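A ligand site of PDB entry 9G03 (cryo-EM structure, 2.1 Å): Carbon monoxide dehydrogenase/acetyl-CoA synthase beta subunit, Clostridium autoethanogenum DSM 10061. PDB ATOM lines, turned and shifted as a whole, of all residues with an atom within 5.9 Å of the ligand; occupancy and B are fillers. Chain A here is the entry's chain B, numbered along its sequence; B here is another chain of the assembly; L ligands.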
ATOM      1  N   HIS A  92      14.535  12.558   7.417  1.00  0.00           N
ATOM      2  CA  HIS A  92      15.193  13.183   8.557  1.00  0.00           C
ATOM      3  C   HIS A  92      16.257  14.199   8.125  1.00  0.00           C
ATOM      4  O   HIS A  92      16.380  15.275   8.713  1.00  0.00           O
ATOM      5  CB  HIS A  92      15.802  12.112   9.451  1.00  0.00           C
ATOM      6  CG  HIS A  92      14.812  11.484  10.379  1.00  0.00           C
ATOM      7  ND1 HIS A  92      14.866  10.156  10.728  1.00  0.00           N
ATOM      8  CD2 HIS A  92      13.733  11.996  11.018  1.00  0.00           C
ATOM      9  CE1 HIS A  92      13.858   9.880  11.550  1.00  0.00           C
ATOM     10  NE2 HIS A  92      13.165  10.990  11.733  1.00  0.00           N
ATOM     11  N   GLY A 257       2.589  17.871  11.770  1.00  0.00           N
ATOM     12  CA  GLY A 257       3.789  17.784  10.951  1.00  0.00           C
ATOM     13  C   GLY A 257       5.070  17.643  11.739  1.00  0.00           C
ATOM     14  O   GLY A 257       5.055  17.108  12.848  1.00  0.00           O
ATOM     15  N   HIS A 258       6.198  18.080  11.164  1.00  0.00           N
ATOM     16  CA  HIS A 258       7.476  17.828  11.801  1.00  0.00           C
ATOM     17  C   HIS A 258       8.394  19.044  11.904  1.00  0.00           C
ATOM     18  O   HIS A 258       9.169  19.133  12.860  1.00  0.00           O
ATOM     19  CB  HIS A 258       8.192  16.702  11.050  1.00  0.00           C
ATOM     20  CG  HIS A 258       7.599  15.351  11.309  1.00  0.00           C
ATOM     21  ND1 HIS A 258       6.376  14.970  10.806  1.00  0.00           N
ATOM     22  CD2 HIS A 258       8.045  14.313  12.053  1.00  0.00           C
ATOM     23  CE1 HIS A 258       6.096  13.747  11.222  1.00  0.00           C
ATOM     24  NE2 HIS A 258       7.091  13.325  11.986  1.00  0.00           N
ATOM     25  N   CYS A 293       1.632  14.965  16.770  1.00  0.00           N
ATOM     26  CA  CYS A 293       2.816  14.272  16.242  1.00  0.00           C
ATOM     27  C   CYS A 293       4.066  15.074  16.636  1.00  0.00           C
ATOM     28  O   CYS A 293       4.131  15.642  17.739  1.00  0.00           O
ATOM     29  CB  CYS A 293       2.644  14.027  14.747  1.00  0.00           C
ATOM     30  SG  CYS A 293       1.390  12.778  14.325  1.00  0.00           S
ATOM     31  N   CYS A 294       5.082  15.152  15.771  1.00  0.00           N
ATOM     32  CA  CYS A 294       6.384  15.657  16.185  1.00  0.00           C
ATOM     33  C   CYS A 294       6.421  17.174  16.321  1.00  0.00           C
ATOM     34  O   CYS A 294       7.094  17.687  17.221  1.00  0.00           O
ATOM     35  CB  CYS A 294       7.456  15.186  15.216  1.00  0.00           C
ATOM     36  SG  CYS A 294       7.954  13.491  15.541  1.00  0.00           S
ATOM     37  N   ASN A 310      -1.544  11.747  18.752  1.00  0.00           N
ATOM     38  CA  ASN A 310      -0.496  11.194  17.892  1.00  0.00           C
ATOM     39  C   ASN A 310      -1.049  10.794  16.513  1.00  0.00           C
ATOM     40  O   ASN A 310      -2.185  11.109  16.151  1.00  0.00           O
ATOM     41  CB  ASN A 310       0.216  10.039  18.607  1.00  0.00           C
ATOM     42  CG  ASN A 310      -0.726   8.998  19.210  1.00  0.00           C
ATOM     43  OD1 ASN A 310      -1.921   8.984  18.948  1.00  0.00           O
ATOM     44  ND2 ASN A 310      -0.162   8.102  20.016  1.00  0.00           N
ATOM     45  N   PHE A 311      -0.263  10.028  15.746  1.00  0.00           N
ATOM     46  CA  PHE A 311      -0.500   9.793  14.318  1.00  0.00           C
ATOM     47  C   PHE A 311      -1.935   9.350  14.047  1.00  0.00           C
ATOM     48  O   PHE A 311      -2.691  10.069  13.388  1.00  0.00           O
ATOM     49  CB  PHE A 311       0.507   8.762  13.793  1.00  0.00           C
ATOM     50  CG  PHE A 311       0.327   8.391  12.330  1.00  0.00           C
ATOM     51  CD1 PHE A 311       0.590   9.315  11.325  1.00  0.00           C
ATOM     52  CD2 PHE A 311      -0.093   7.126  11.969  1.00  0.00           C
ATOM     53  CE1 PHE A 311       0.434   8.968   9.980  1.00  0.00           C
ATOM     54  CE2 PHE A 311      -0.248   6.780  10.624  1.00  0.00           C
ATOM     55  CZ  PHE A 311       0.010   7.704   9.639  1.00  0.00           C
ATOM     56  N   GLN A 331       5.350  15.308   6.258  1.00  0.00           N
ATOM     57  CA  GLN A 331       5.591  13.999   6.873  1.00  0.00           C
ATOM     58  C   GLN A 331       4.446  13.557   7.792  1.00  0.00           C
ATOM     59  O   GLN A 331       3.990  14.322   8.632  1.00  0.00           O
ATOM     60  CB  GLN A 331       6.916  13.999   7.666  1.00  0.00           C
ATOM     61  CG  GLN A 331       8.168  14.250   6.817  1.00  0.00           C
ATOM     62  CD  GLN A 331       9.449  14.244   7.642  1.00  0.00           C
ATOM     63  OE1 GLN A 331       9.506  13.658   8.717  1.00  0.00           O
ATOM     64  NE2 GLN A 331      10.484  14.904   7.132  1.00  0.00           N
ATOM     65  N   CYS A 332       3.999  12.312   7.619  1.00  0.00           N
ATOM     66  CA  CYS A 332       2.981  11.683   8.480  1.00  0.00           C
ATOM     67  C   CYS A 332       1.671  12.464   8.527  1.00  0.00           C
ATOM     68  O   CYS A 332       0.940  12.422   9.515  1.00  0.00           O
ATOM     69  CB  CYS A 332       3.529  11.483   9.898  1.00  0.00           C
ATOM     70  SG  CYS A 332       5.102  10.567   9.933  1.00  0.00           S
ATOM     71  N   VAL A 448       9.984   4.270  21.092  1.00  0.00           N
ATOM     72  CA  VAL A 448       9.841   5.217  19.987  1.00  0.00           C
ATOM     73  C   VAL A 448       8.889   4.606  18.967  1.00  0.00           C
ATOM     74  O   VAL A 448       8.539   3.431  19.049  1.00  0.00           O
ATOM     75  CB  VAL A 448      11.205   5.536  19.324  1.00  0.00           C
ATOM     76  CG1 VAL A 448      12.243   5.886  20.372  1.00  0.00           C
ATOM     77  CG2 VAL A 448      11.660   4.361  18.477  1.00  0.00           C
ATOM     78  N   GLY A 449       8.458   5.412  18.018  1.00  0.00           N
ATOM     79  CA  GLY A 449       7.734   4.879  16.882  1.00  0.00           C
ATOM     80  C   GLY A 449       6.324   5.417  16.791  1.00  0.00           C
ATOM     81  O   GLY A 449       5.831   6.126  17.665  1.00  0.00           O
ATOM     82  N   CYS A 450       5.646   4.964  15.744  1.00  0.00           N
ATOM     83  CA  CYS A 450       4.336   5.443  15.360  1.00  0.00           C
ATOM     84  C   CYS A 450       3.236   4.544  15.893  1.00  0.00           C
ATOM     85  O   CYS A 450       3.458   3.739  16.807  1.00  0.00           O
ATOM     86  CB  CYS A 450       4.290   5.394  13.825  1.00  0.00           C
ATOM     87  SG  CYS A 450       5.920   5.521  13.001  1.00  0.00           S
ATOM     88  N   ASN A 451       2.033   4.728  15.378  1.00  0.00           N
ATOM     89  CA  ASN A 451       0.945   3.767  15.495  1.00  0.00           C
ATOM     90  C   ASN A 451       0.874   2.989  14.182  1.00  0.00           C
ATOM     91  O   ASN A 451       1.500   3.350  13.192  1.00  0.00           O
ATOM     92  CB  ASN A 451      -0.396   4.463  15.784  1.00  0.00           C
ATOM     93  CG  ASN A 451      -0.365   5.290  17.046  1.00  0.00           C
ATOM     94  OD1 ASN A 451      -0.691   6.475  17.010  1.00  0.00           O
ATOM     95  ND2 ASN A 451       0.032   4.687  18.155  1.00  0.00           N
ATOM     96  N   THR A 478       9.956   8.966  22.817  1.00  0.00           N
ATOM     97  CA  THR A 478       9.892  10.007  21.788  1.00  0.00           C
ATOM     98  C   THR A 478       8.700   9.769  20.878  1.00  0.00           C
ATOM     99  O   THR A 478       8.155   8.662  20.792  1.00  0.00           O
ATOM    100  CB  THR A 478      11.162  10.074  20.918  1.00  0.00           C
ATOM    101  OG1 THR A 478      11.271   8.890  20.128  1.00  0.00           O
ATOM    102  CG2 THR A 478      12.407  10.225  21.781  1.00  0.00           C
ATOM    103  N   GLY A 479       8.270  10.845  20.228  1.00  0.00           N
ATOM    104  CA  GLY A 479       7.314  10.748  19.140  1.00  0.00           C
ATOM    105  C   GLY A 479       5.932  10.303  19.588  1.00  0.00           C
ATOM    106  O   GLY A 479       5.424  10.678  20.653  1.00  0.00           O
ATOM    107  N   CYS A 480       5.292   9.508  18.724  1.00  0.00           N
ATOM    108  CA  CYS A 480       3.937   9.072  18.982  1.00  0.00           C
ATOM    109  C   CYS A 480       3.868   8.130  20.194  1.00  0.00           C
ATOM    110  O   CYS A 480       2.852   8.112  20.893  1.00  0.00           O
ATOM    111  CB  CYS A 480       3.355   8.421  17.727  1.00  0.00           C
ATOM    112  SG  CYS A 480       2.967   9.620  16.427  1.00  0.00           S
ATOM    113  N   ALA A 481       4.922   7.361  20.449  1.00  0.00           N
ATOM    114  CA  ALA A 481       4.986   6.581  21.685  1.00  0.00           C
ATOM    115  C   ALA A 481       4.990   7.485  22.908  1.00  0.00           C
ATOM    116  O   ALA A 481       4.281   7.223  23.887  1.00  0.00           O
ATOM    117  CB  ALA A 481       6.230   5.689  21.668  1.00  0.00           C
ATOM    118  N   SER A 521      10.791  14.842  19.995  1.00  0.00           N
ATOM    119  CA  SER A 521      10.270  14.331  18.728  1.00  0.00           C
ATOM    120  C   SER A 521      11.150  13.182  18.219  1.00  0.00           C
ATOM    121  O   SER A 521      12.080  12.744  18.887  1.00  0.00           O
ATOM    122  CB  SER A 521      10.186  15.449  17.692  1.00  0.00           C
ATOM    123  OG  SER A 521      11.478  15.920  17.358  1.00  0.00           O
ATOM    124  N   CYS A 522      10.874  12.734  16.994  1.00  0.00           N
ATOM    125  CA  CYS A 522      11.632  11.633  16.416  1.00  0.00           C
ATOM    126  C   CYS A 522      13.095  12.005  16.162  1.00  0.00           C
ATOM    127  O   CYS A 522      13.995  11.195  16.395  1.00  0.00           O
ATOM    128  CB  CYS A 522      10.965  11.160  15.126  1.00  0.00           C
ATOM    129  SG  CYS A 522       9.431  10.331  15.460  1.00  0.00           S
ATOM    130  N   MET A 556       5.405   2.437  11.773  1.00  0.00           N
ATOM    131  CA  MET A 556       4.853   2.342  10.426  1.00  0.00           C
ATOM    132  C   MET A 556       5.746   2.952   9.344  1.00  0.00           C
ATOM    133  O   MET A 556       5.719   2.496   8.204  1.00  0.00           O
ATOM    134  CB  MET A 556       3.456   2.973  10.376  1.00  0.00           C
ATOM    135  CG  MET A 556       3.417   4.497  10.495  1.00  0.00           C
ATOM    136  SD  MET A 556       3.524   5.422   8.944  1.00  0.00           S
ATOM    137  CE  MET A 556       3.579   7.095   9.591  1.00  0.00           C
ATOM    138  N   SER A 557       6.526   3.978   9.678  1.00  0.00           N
ATOM    139  CA  SER A 557       7.161   4.827   8.686  1.00  0.00           C
ATOM    140  C   SER A 557       8.539   4.290   8.267  1.00  0.00           C
ATOM    141  O   SER A 557       9.186   3.539   8.996  1.00  0.00           O
ATOM    142  CB  SER A 557       7.290   6.269   9.192  1.00  0.00           C
ATOM    143  OG  SER A 557       8.145   6.361  10.310  1.00  0.00           O
ATOM    144  N   LYS A 559      10.969   6.275   8.167  1.00  0.00           N
ATOM    145  CA  LYS A 559      11.806   6.916   9.182  1.00  0.00           C
ATOM    146  C   LYS A 559      12.049   5.984  10.359  1.00  0.00           C
ATOM    147  O   LYS A 559      13.177   5.907  10.856  1.00  0.00           O
ATOM    148  CB  LYS A 559      11.148   8.204   9.674  1.00  0.00           C
ATOM    149  CG  LYS A 559      11.349   9.394   8.791  1.00  0.00           C
ATOM    150  CD  LYS A 559      10.700  10.641   9.368  1.00  0.00           C
ATOM    151  CE  LYS A 559       9.171  10.525   9.374  1.00  0.00           C
ATOM    152  NZ  LYS A 559       8.462  11.662  10.023  1.00  0.00           N
ATOM    153  N   ALA A 560      11.034   5.236  10.774  1.00  0.00           N
ATOM    154  CA  ALA A 560      11.209   4.274  11.866  1.00  0.00           C
ATOM    155  C   ALA A 560      12.218   3.198  11.495  1.00  0.00           C
ATOM    156  O   ALA A 560      13.024   2.780  12.331  1.00  0.00           O
ATOM    157  CB  ALA A 560       9.869   3.657  12.246  1.00  0.00           C
ATOM    158  N   ILE A 563      15.617   4.679  11.746  1.00  0.00           N
ATOM    159  CA  ILE A 563      15.939   4.877  13.153  1.00  0.00           C
ATOM    160  C   ILE A 563      16.401   3.560  13.786  1.00  0.00           C
ATOM    161  O   ILE A 563      17.447   3.509  14.427  1.00  0.00           O
ATOM    162  CB  ILE A 563      14.732   5.450  13.915  1.00  0.00           C
ATOM    163  CG1 ILE A 563      14.513   6.929  13.566  1.00  0.00           C
ATOM    164  CG2 ILE A 563      14.911   5.314  15.434  1.00  0.00           C
ATOM    165  CD1 ILE A 563      13.160   7.430  13.970  1.00  0.00           C
ATOM    166  N   HIS B 194       7.852  10.002   0.967  1.00  0.00           N
ATOM    167  CA  HIS B 194       7.614   9.369   2.265  1.00  0.00           C
ATOM    168  C   HIS B 194       6.137   9.482   2.665  1.00  0.00           C
ATOM    169  O   HIS B 194       5.454  10.442   2.301  1.00  0.00           O
ATOM    170  CB  HIS B 194       8.494  10.046   3.319  1.00  0.00           C
ATOM    171  CG  HIS B 194       8.431   9.412   4.677  1.00  0.00           C
ATOM    172  ND1 HIS B 194       7.417   9.654   5.573  1.00  0.00           N
ATOM    173  CD2 HIS B 194       9.293   8.578   5.311  1.00  0.00           C
ATOM    174  CE1 HIS B 194       7.639   8.982   6.687  1.00  0.00           C
ATOM    175  NE2 HIS B 194       8.764   8.315   6.555  1.00  0.00           N
HETATM  176 FE1  LIG L   1       5.393   9.997  12.186  1.00  0.00          FE
HETATM  177 FE2  LIG L   1       7.443  12.229  13.685  1.00  0.00          FE
HETATM  178 FE3  LIG L   1       6.017   7.732  13.437  1.00  0.00          FE
HETATM  179 FE4  LIG L   1       4.625   9.594  14.908  1.00  0.00          FE
HETATM  180  S1  LIG L   1       6.659   8.623  15.446  1.00  0.00           S
HETATM  181  S2  LIG L   1       3.881   8.411  13.029  1.00  0.00           S
HETATM  182  S3  LIG L   1       7.406   8.869  11.925  1.00  0.00           S
HETATM  183  S4  LIG L   1       5.192  11.564  13.764  1.00  0.00           S
HETATM  184 NI1  LIG L   1       8.020   9.812  14.028  1.00  0.00          NI
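O of Gly 449 lies close to S1 of the ligand, 3.4 Å away.
Merely in contact with the ligand: Cys 293 (3.7 Å), Phe 311 (3.5 Å) and Met 556 (3.7 Å).
Hydrophobic or aromatic side chains within 4 Å of the ligand: His 258, Phe 311 and Met 556.
12 residues have an atom within 4 Å of the ligand: His 258, Cys 293, Cys 294, Phe 311, Cys 332, Gly 449, Cys 450, Cys 480, Cys 522, Met 556, Ser 557 and Lys 559.
NZ of Lys 559 lies close to SG of Cys 332, 3.5 Å away.
The backbone carbonyl oxygen of Cys 480 sits at hydrogen-bond distance from the side-chain amide nitrogen of Asn 310 (3.1 Å).
The backbone NH of Lys 559 is in hydrogen-bond range of a ring nitrogen (NE2) of His 194 of chain B, at 3.4 Å.
O of Gln 331 is in hydrogen-bond range of ND1 of His 258, at 3.3 Å.
The side-chain amino group (NZ) of Lys 559 lies within hydrogen-bond range of the side-chain amide oxygen (OE1) of Gln 331, at 2.6 Å.
SG of Cys 450 sits close to N of Met 556, at 3.4 Å.
NE2 of His 258 sits close to NZ of Lys 559 (2.9 Å).
The backbone NH (N) of Ala 481 sits at hydrogen-bond distance from the backbone carbonyl oxygen (O) of Gly 449 (3.2 Å).
NE2 of His 258 binds FE2 of the ligand.
The side-chain sulfur (SG) of Cys 522 is bound to a nickel atom (NI1) of the ligand (2.1 Å).
An iron atom (FE4) of the ligand is bound by the side-chain sulfur (SG) of Cys 480 (2.2 Å).
The side-chain hydroxyl of Ser 557 sits close to a sulfur (S3) of the ligand (3.1 Å).
SG of Cys 332 is bound to FE1 of the ligand (2.3 Å).
An iron atom (FE2) of the ligand is bound by the side-chain sulfur (SG) of Cys 294 (2.3 Å).
SG of Cys 450 binds FE3 of the ligand, 2.3 Å away.
The backbone NH (N) of Cys 480 sits close to a sulfur (S1) of the ligand (3.7 Å).
A sulfur (S3) of the ligand sits close to the side-chain amino group of Lys 559 (3.5 Å).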
